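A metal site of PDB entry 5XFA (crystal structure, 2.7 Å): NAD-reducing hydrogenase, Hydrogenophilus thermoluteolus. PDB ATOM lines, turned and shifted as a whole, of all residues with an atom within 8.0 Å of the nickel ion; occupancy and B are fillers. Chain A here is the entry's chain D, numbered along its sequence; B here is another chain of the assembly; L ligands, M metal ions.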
ATOM      1  N   GLU A  32     -29.262 -16.617  -4.276  1.00  0.00           N
ATOM      2  CA  GLU A  32     -29.730 -17.422  -3.168  1.00  0.00           C
ATOM      3  C   GLU A  32     -30.803 -16.630  -2.463  1.00  0.00           C
ATOM      4  O   GLU A  32     -30.739 -15.395  -2.388  1.00  0.00           O
ATOM      5  CB  GLU A  32     -28.588 -17.931  -2.268  1.00  0.00           C
ATOM      6  CG  GLU A  32     -28.370 -17.201  -0.954  1.00  0.00           C
ATOM      7  CD  GLU A  32     -29.503 -17.333   0.054  1.00  0.00           C
ATOM      8  OE1 GLU A  32     -30.177 -16.315   0.299  1.00  0.00           O
ATOM      9  OE2 GLU A  32     -29.700 -18.402   0.649  1.00  0.00           O
ATOM     10  N   GLN A  77     -25.550 -20.592  12.159  1.00  0.00           N
ATOM     11  CA  GLN A  77     -25.013 -20.771  10.794  1.00  0.00           C
ATOM     12  C   GLN A  77     -26.035 -21.346   9.800  1.00  0.00           C
ATOM     13  O   GLN A  77     -25.802 -21.365   8.598  1.00  0.00           O
ATOM     14  CB  GLN A  77     -23.730 -21.626  10.786  1.00  0.00           C
ATOM     15  CG  GLN A  77     -23.937 -23.052  11.227  1.00  0.00           C
ATOM     16  CD  GLN A  77     -22.697 -23.904  11.074  1.00  0.00           C
ATOM     17  OE1 GLN A  77     -21.800 -23.604  10.269  1.00  0.00           O
ATOM     18  NE2 GLN A  77     -22.651 -24.987  11.850  1.00  0.00           N
ATOM     19  N   LEU A  79     -28.485 -19.862   8.948  1.00  0.00           N
ATOM     20  CA  LEU A  79     -28.884 -18.704   8.123  1.00  0.00           C
ATOM     21  C   LEU A  79     -28.667 -18.951   6.635  1.00  0.00           C
ATOM     22  O   LEU A  79     -29.474 -18.525   5.810  1.00  0.00           O
ATOM     23  CB  LEU A  79     -28.087 -17.431   8.475  1.00  0.00           C
ATOM     24  CG  LEU A  79     -28.383 -16.561   9.714  1.00  0.00           C
ATOM     25  CD1 LEU A  79     -27.988 -15.109   9.471  1.00  0.00           C
ATOM     26  CD2 LEU A  79     -29.830 -16.651  10.123  1.00  0.00           C
ATOM     27  N   CYS A  80     -27.568 -19.617   6.292  1.00  0.00           N
ATOM     28  CA  CYS A  80     -27.205 -19.749   4.933  1.00  0.00           C
ATOM     29  C   CYS A  80     -26.367 -20.971   4.681  1.00  0.00           C
ATOM     30  O   CYS A  80     -25.484 -21.314   5.447  1.00  0.00           O
ATOM     31  CB  CYS A  80     -26.451 -18.478   4.484  1.00  0.00           C
ATOM     32  SG  CYS A  80     -25.878 -18.552   2.782  1.00  0.00           S
ATOM     33  N   GLY A  81     -26.622 -21.595   3.539  1.00  0.00           N
ATOM     34  CA  GLY A  81     -25.939 -22.815   3.116  1.00  0.00           C
ATOM     35  C   GLY A  81     -24.833 -22.564   2.133  1.00  0.00           C
ATOM     36  O   GLY A  81     -24.166 -23.523   1.715  1.00  0.00           O
ATOM     37  N   ILE A  82     -24.596 -21.300   1.787  1.00  0.00           N
ATOM     38  CA  ILE A  82     -23.361 -20.957   1.083  1.00  0.00           C
ATOM     39  C   ILE A  82     -22.253 -20.483   2.033  1.00  0.00           C
ATOM     40  O   ILE A  82     -21.099 -20.873   1.919  1.00  0.00           O
ATOM     41  CB  ILE A  82     -23.594 -19.969  -0.078  1.00  0.00           C
ATOM     42  CG1 ILE A  82     -24.695 -20.488  -1.016  1.00  0.00           C
ATOM     43  CG2 ILE A  82     -22.319 -19.807  -0.888  1.00  0.00           C
ATOM     44  CD1 ILE A  82     -25.282 -19.441  -1.920  1.00  0.00           C
ATOM     45  N   CYS A  83     -22.584 -19.674   3.017  1.00  0.00           N
ATOM     46  CA  CYS A  83     -21.575 -19.163   3.920  1.00  0.00           C
ATOM     47  C   CYS A  83     -21.877 -19.525   5.406  1.00  0.00           C
ATOM     48  O   CYS A  83     -21.646 -18.737   6.335  1.00  0.00           O
ATOM     49  CB  CYS A  83     -21.432 -17.655   3.687  1.00  0.00           C
ATOM     50  SG  CYS A  83     -22.952 -16.753   4.007  1.00  0.00           S
ATOM     51  N   PRO A  84     -22.335 -20.733   5.663  1.00  0.00           N
ATOM     52  CA  PRO A  84     -22.456 -20.978   7.049  1.00  0.00           C
ATOM     53  C   PRO A  84     -21.124 -20.775   7.768  1.00  0.00           C
ATOM     54  O   PRO A  84     -21.118 -20.438   8.972  1.00  0.00           O
ATOM     55  CB  PRO A  84     -22.879 -22.436   7.109  1.00  0.00           C
ATOM     56  CG  PRO A  84     -22.258 -23.024   5.892  1.00  0.00           C
ATOM     57  CD  PRO A  84     -22.384 -21.963   4.872  1.00  0.00           C
ATOM     58  N   VAL A  85     -20.003 -20.998   7.090  1.00  0.00           N
ATOM     59  CA  VAL A  85     -18.710 -20.851   7.787  1.00  0.00           C
ATOM     60  C   VAL A  85     -18.510 -19.443   8.323  1.00  0.00           C
ATOM     61  O   VAL A  85     -17.981 -19.252   9.421  1.00  0.00           O
ATOM     62  CB  VAL A  85     -17.520 -21.219   6.900  1.00  0.00           C
ATOM     63  CG1 VAL A  85     -16.238 -20.763   7.559  1.00  0.00           C
ATOM     64  CG2 VAL A  85     -17.500 -22.726   6.668  1.00  0.00           C
ATOM     65  N   SER A  86     -18.964 -18.463   7.544  1.00  0.00           N
ATOM     66  CA  SER A  86     -18.884 -17.058   7.954  1.00  0.00           C
ATOM     67  C   SER A  86     -19.656 -16.827   9.249  1.00  0.00           C
ATOM     68  O   SER A  86     -19.186 -16.105  10.085  1.00  0.00           O
ATOM     69  CB  SER A  86     -19.378 -16.121   6.834  1.00  0.00           C
ATOM     70  OG  SER A  86     -18.499 -16.158   5.714  1.00  0.00           O
ATOM     71  N   HIS A  87     -20.793 -17.476   9.430  1.00  0.00           N
ATOM     72  CA  HIS A  87     -21.566 -17.311  10.661  1.00  0.00           C
ATOM     73  C   HIS A  87     -21.051 -18.164  11.789  1.00  0.00           C
ATOM     74  O   HIS A  87     -21.192 -17.826  12.957  1.00  0.00           O
ATOM     75  CB  HIS A  87     -23.053 -17.647  10.415  1.00  0.00           C
ATOM     76  CG  HIS A  87     -23.700 -16.753   9.425  1.00  0.00           C
ATOM     77  ND1 HIS A  87     -24.391 -15.627   9.789  1.00  0.00           N
ATOM     78  CD2 HIS A  87     -23.656 -16.767   8.078  1.00  0.00           C
ATOM     79  CE1 HIS A  87     -24.790 -14.999   8.687  1.00  0.00           C
ATOM     80  NE2 HIS A  87     -24.348 -15.672   7.639  1.00  0.00           N
ATOM     81  N   GLN A 119     -13.885 -21.357   2.503  1.00  0.00           N
ATOM     82  CA  GLN A 119     -15.264 -20.847   2.383  1.00  0.00           C
ATOM     83  C   GLN A 119     -15.367 -19.780   1.301  1.00  0.00           C
ATOM     84  O   GLN A 119     -16.278 -19.816   0.494  1.00  0.00           O
ATOM     85  CB  GLN A 119     -15.786 -20.303   3.728  1.00  0.00           C
ATOM     86  CG  GLN A 119     -17.225 -19.827   3.593  1.00  0.00           C
ATOM     87  CD  GLN A 119     -17.496 -18.508   4.307  1.00  0.00           C
ATOM     88  OE1 GLN A 119     -16.614 -17.906   4.943  1.00  0.00           O
ATOM     89  NE2 GLN A 119     -18.722 -18.038   4.190  1.00  0.00           N
ATOM     90  N   SER A 123     -17.367 -20.204  -2.295  1.00  0.00           N
ATOM     91  CA  SER A 123     -18.540 -19.351  -2.434  1.00  0.00           C
ATOM     92  C   SER A 123     -18.390 -18.471  -3.640  1.00  0.00           C
ATOM     93  O   SER A 123     -19.340 -18.230  -4.368  1.00  0.00           O
ATOM     94  CB  SER A 123     -18.799 -18.479  -1.194  1.00  0.00           C
ATOM     95  OG  SER A 123     -19.805 -17.504  -1.483  1.00  0.00           O
ATOM     96  N   ALA A 394     -17.130 -11.857   5.426  1.00  0.00           N
ATOM     97  CA  ALA A 394     -17.755 -12.990   4.790  1.00  0.00           C
ATOM     98  C   ALA A 394     -17.582 -12.816   3.283  1.00  0.00           C
ATOM     99  O   ALA A 394     -17.151 -11.759   2.855  1.00  0.00           O
ATOM    100  CB  ALA A 394     -19.205 -13.046   5.158  1.00  0.00           C
ATOM    101  N   PRO A 395     -17.879 -13.841   2.481  1.00  0.00           N
ATOM    102  CA  PRO A 395     -17.631 -13.672   1.057  1.00  0.00           C
ATOM    103  C   PRO A 395     -18.255 -12.424   0.465  1.00  0.00           C
ATOM    104  O   PRO A 395     -17.581 -11.709  -0.267  1.00  0.00           O
ATOM    105  CB  PRO A 395     -18.260 -14.940   0.461  1.00  0.00           C
ATOM    106  CG  PRO A 395     -18.029 -15.972   1.498  1.00  0.00           C
ATOM    107  CD  PRO A 395     -18.201 -15.246   2.801  1.00  0.00           C
ATOM    108  N   ARG A 396     -19.512 -12.157   0.834  1.00  0.00           N
ATOM    109  CA  ARG A 396     -20.322 -11.079   0.249  1.00  0.00           C
ATOM    110  C   ARG A 396     -20.220  -9.727   0.973  1.00  0.00           C
ATOM    111  O   ARG A 396     -20.986  -8.830   0.694  1.00  0.00           O
ATOM    112  CB  ARG A 396     -21.785 -11.506   0.199  1.00  0.00           C
ATOM    113  CG  ARG A 396     -22.013 -12.681  -0.752  1.00  0.00           C
ATOM    114  CD  ARG A 396     -23.277 -13.497  -0.422  1.00  0.00           C
ATOM    115  NE  ARG A 396     -23.459 -14.646  -1.319  1.00  0.00           N
ATOM    116  CZ  ARG A 396     -22.669 -15.727  -1.358  1.00  0.00           C
ATOM    117  NH1 ARG A 396     -22.948 -16.701  -2.219  1.00  0.00           N
ATOM    118  NH2 ARG A 396     -21.591 -15.854  -0.592  1.00  0.00           N
ATOM    119  N   VAL A 418     -25.844  -8.580   8.606  1.00  0.00           N
ATOM    120  CA  VAL A 418     -25.260  -9.517   7.642  1.00  0.00           C
ATOM    121  C   VAL A 418     -24.858  -8.862   6.326  1.00  0.00           C
ATOM    122  O   VAL A 418     -25.509  -7.922   5.893  1.00  0.00           O
ATOM    123  CB  VAL A 418     -26.232 -10.649   7.399  1.00  0.00           C
ATOM    124  CG1 VAL A 418     -25.783 -11.516   6.237  1.00  0.00           C
ATOM    125  CG2 VAL A 418     -26.396 -11.467   8.685  1.00  0.00           C
ATOM    126  N   SER A 419     -23.771  -9.357   5.717  1.00  0.00           N
ATOM    127  CA  SER A 419     -23.117  -8.717   4.536  1.00  0.00           C
ATOM    128  C   SER A 419     -24.099  -8.142   3.560  1.00  0.00           C
ATOM    129  O   SER A 419     -24.065  -6.955   3.307  1.00  0.00           O
ATOM    130  CB  SER A 419     -22.152  -9.643   3.729  1.00  0.00           C
ATOM    131  OG  SER A 419     -21.636 -10.725   4.468  1.00  0.00           O
ATOM    132  N   THR A 420     -24.980  -8.965   3.010  1.00  0.00           N
ATOM    133  CA  THR A 420     -25.857  -8.477   1.957  1.00  0.00           C
ATOM    134  C   THR A 420     -26.759  -7.337   2.453  1.00  0.00           C
ATOM    135  O   THR A 420     -26.980  -6.357   1.739  1.00  0.00           O
ATOM    136  CB  THR A 420     -26.675  -9.587   1.283  1.00  0.00           C
ATOM    137  OG1 THR A 420     -25.869 -10.207   0.265  1.00  0.00           O
ATOM    138  CG2 THR A 420     -27.940  -9.034   0.635  1.00  0.00           C
ATOM    139  N   ASP A 460     -23.809 -10.819  -5.926  1.00  0.00           N
ATOM    140  CA  ASP A 460     -23.935 -12.128  -5.267  1.00  0.00           C
ATOM    141  C   ASP A 460     -24.819 -11.964  -4.062  1.00  0.00           C
ATOM    142  O   ASP A 460     -24.353 -12.085  -2.928  1.00  0.00           O
ATOM    143  CB  ASP A 460     -22.547 -12.638  -4.831  1.00  0.00           C
ATOM    144  CG  ASP A 460     -22.524 -14.131  -4.438  1.00  0.00           C
ATOM    145  OD1 ASP A 460     -23.520 -14.870  -4.649  1.00  0.00           O
ATOM    146  OD2 ASP A 460     -21.467 -14.563  -3.968  1.00  0.00           O
ATOM    147  N   PRO A 461     -26.093 -11.648  -4.274  1.00  0.00           N
ATOM    148  CA  PRO A 461     -26.924 -11.401  -3.110  1.00  0.00           C
ATOM    149  C   PRO A 461     -27.277 -12.696  -2.374  1.00  0.00           C
ATOM    150  O   PRO A 461     -27.749 -13.658  -2.991  1.00  0.00           O
ATOM    151  CB  PRO A 461     -28.184 -10.758  -3.691  1.00  0.00           C
ATOM    152  CG  PRO A 461     -27.981 -10.670  -5.155  1.00  0.00           C
ATOM    153  CD  PRO A 461     -26.861 -11.570  -5.521  1.00  0.00           C
ATOM    154  N   CYS A 462     -27.049 -12.705  -1.059  1.00  0.00           N
ATOM    155  CA  CYS A 462     -27.511 -13.780  -0.205  1.00  0.00           C
ATOM    156  C   CYS A 462     -28.660 -13.275   0.643  1.00  0.00           C
ATOM    157  O   CYS A 462     -28.452 -12.562   1.628  1.00  0.00           O
ATOM    158  CB  CYS A 462     -26.371 -14.291   0.680  1.00  0.00           C
ATOM    159  SG  CYS A 462     -26.637 -15.965   1.293  1.00  0.00           S
ATOM    160  N   LEU A 463     -29.877 -13.626   0.249  1.00  0.00           N
ATOM    161  CA  LEU A 463     -31.081 -12.975   0.791  1.00  0.00           C
ATOM    162  C   LEU A 463     -31.551 -13.640   2.090  1.00  0.00           C
ATOM    163  O   LEU A 463     -32.085 -12.961   2.979  1.00  0.00           O
ATOM    164  CB  LEU A 463     -32.174 -12.950  -0.270  1.00  0.00           C
ATOM    165  CG  LEU A 463     -31.700 -12.261  -1.566  1.00  0.00           C
ATOM    166  CD1 LEU A 463     -32.687 -12.394  -2.709  1.00  0.00           C
ATOM    167  CD2 LEU A 463     -31.400 -10.785  -1.307  1.00  0.00           C
ATOM    168  N   SER A 464     -31.300 -14.948   2.221  1.00  0.00           N
ATOM    169  CA  SER A 464     -31.484 -15.652   3.496  1.00  0.00           C
ATOM    170  C   SER A 464     -30.578 -15.039   4.545  1.00  0.00           C
ATOM    171  O   SER A 464     -30.981 -14.781   5.664  1.00  0.00           O
ATOM    172  CB  SER A 464     -31.142 -17.136   3.348  1.00  0.00           C
ATOM    173  OG  SER A 464     -31.831 -17.728   2.262  1.00  0.00           O
ATOM    174  N   CYS A 465     -29.343 -14.836   4.169  1.00  0.00           N
ATOM    175  CA  CYS A 465     -28.388 -14.168   5.038  1.00  0.00           C
ATOM    176  C   CYS A 465     -28.893 -12.802   5.400  1.00  0.00           C
ATOM    177  O   CYS A 465     -28.866 -12.413   6.557  1.00  0.00           O
ATOM    178  CB  CYS A 465     -27.029 -14.035   4.334  1.00  0.00           C
ATOM    179  SG  CYS A 465     -25.853 -15.310   4.780  1.00  0.00           S
ATOM    180  N   ALA A 466     -29.358 -12.084   4.390  1.00  0.00           N
ATOM    181  CA  ALA A 466     -29.702 -10.672   4.519  1.00  0.00           C
ATOM    182  C   ALA A 466     -30.825 -10.376   5.506  1.00  0.00           C
ATOM    183  O   ALA A 466     -30.850  -9.309   6.128  1.00  0.00           O
ATOM    184  CB  ALA A 466     -30.087 -10.122   3.158  1.00  0.00           C
ATOM    185  N   CYS B  24     -32.362 -22.710   3.888  1.00  0.00           N
ATOM    186  CA  CYS B  24     -31.163 -21.879   3.882  1.00  0.00           C
ATOM    187  C   CYS B  24     -30.361 -21.973   2.558  1.00  0.00           C
ATOM    188  O   CYS B  24     -29.273 -21.405   2.446  1.00  0.00           O
ATOM    189  CB  CYS B  24     -30.290 -22.242   5.057  1.00  0.00           C
ATOM    190  SG  CYS B  24     -29.236 -23.680   4.785  1.00  0.00           S
ATOM    191  N   PHE B  25     -30.912 -22.655   1.549  1.00  0.00           N
ATOM    192  CA  PHE B  25     -30.212 -22.925   0.293  1.00  0.00           C
ATOM    193  C   PHE B  25     -29.187 -24.039   0.481  1.00  0.00           C
ATOM    194  O   PHE B  25     -28.493 -24.434  -0.512  1.00  0.00           O
ATOM    195  CB  PHE B  25     -29.534 -21.686  -0.248  1.00  0.00           C
ATOM    196  CG  PHE B  25     -29.353 -21.698  -1.753  1.00  0.00           C
ATOM    197  CD1 PHE B  25     -30.458 -21.623  -2.595  1.00  0.00           C
ATOM    198  CD2 PHE B  25     -28.075 -21.736  -2.307  1.00  0.00           C
ATOM    199  CE1 PHE B  25     -30.281 -21.619  -3.971  1.00  0.00           C
ATOM    200  CE2 PHE B  25     -27.921 -21.731  -3.666  1.00  0.00           C
ATOM    201  CZ  PHE B  25     -29.017 -21.678  -4.506  1.00  0.00           C
HETATM  202 FE1  LIG L   1     -23.760 -14.552   4.062  1.00  0.00          FE
HETATM  203  C1  LIG L   1     -24.299 -13.125   3.108  1.00  0.00           C
HETATM  204  N1  LIG L   1     -24.628 -12.207   2.491  1.00  0.00           N
HETATM  205  C2  LIG L   1     -22.446 -14.120   2.929  1.00  0.00           C
HETATM  206  N2  LIG L   1     -21.603 -13.904   2.164  1.00  0.00           N
HETATM  207  C3  LIG L   1     -23.058 -13.663   5.424  1.00  0.00           C
HETATM  208  O1  LIG L   1     -22.625 -13.149   6.343  1.00  0.00           O
HETATM  209 NI    NI M   1     -24.981 -16.391   2.896  1.00  0.00          NI
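The nickel ion is bound by SG of Cys 465 (2.3 Å). The side-chain sulfur (SG) of Cys 83 binds the nickel ion. The nickel ion is bound by SG of Cys 80, 2.3 Å away. SG of Cys 462 binds the nickel ion (2.3 Å).
FE1 of the ligand is bound by SG of Cys 465 (2.3 Å). An iron atom (FE1) of the ligand is bound by the side-chain sulfur (SG) of Cys 83, at 2.3 Å. N of Arg 396 sits at hydrogen-bond distance from N2 of the ligand, 3.0 Å away. A nitrogen (N2) of the ligand lies close to the guanidinium group (NH2) of Arg 396 (3.4 Å). A ring nitrogen (NE2) of His 87 sits close to an oxygen (O1) of the ligand, 3.3 Å away. The side-chain hydroxyl of Ser 419 is in hydrogen-bond range of an oxygen (O1) of the ligand, 3.2 Å away. N1 of the ligand sits at hydrogen-bond distance from N of Thr 420 (3.3 Å). A nitrogen (N1) of the ligand lies within hydrogen-bond range of the side-chain hydroxyl (OG1) of Thr 420 (3.2 Å).
The side-chain sulfur (SG) of Cys 465 lies close to a ring nitrogen (NE2) of His 87 (3.3 Å). N of Ile 82 lies close to SG of Cys 80 (3.2 Å). The side-chain sulfur (SG) of Cys 462 sits close to the side-chain carboxylate (OE1) of Glu 32, 3.7 Å away. The backbone NH (N) of Cys 462 sits at hydrogen-bond distance from the side-chain hydroxyl (OG1) of Thr 420 (3.1 Å).
Within 4 Å of the nickel ion: Cys 80, Cys 83, Cys 462 and Cys 465. Along chain A the residues within 4 Å of the nickel ion span positions 80 to 465.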
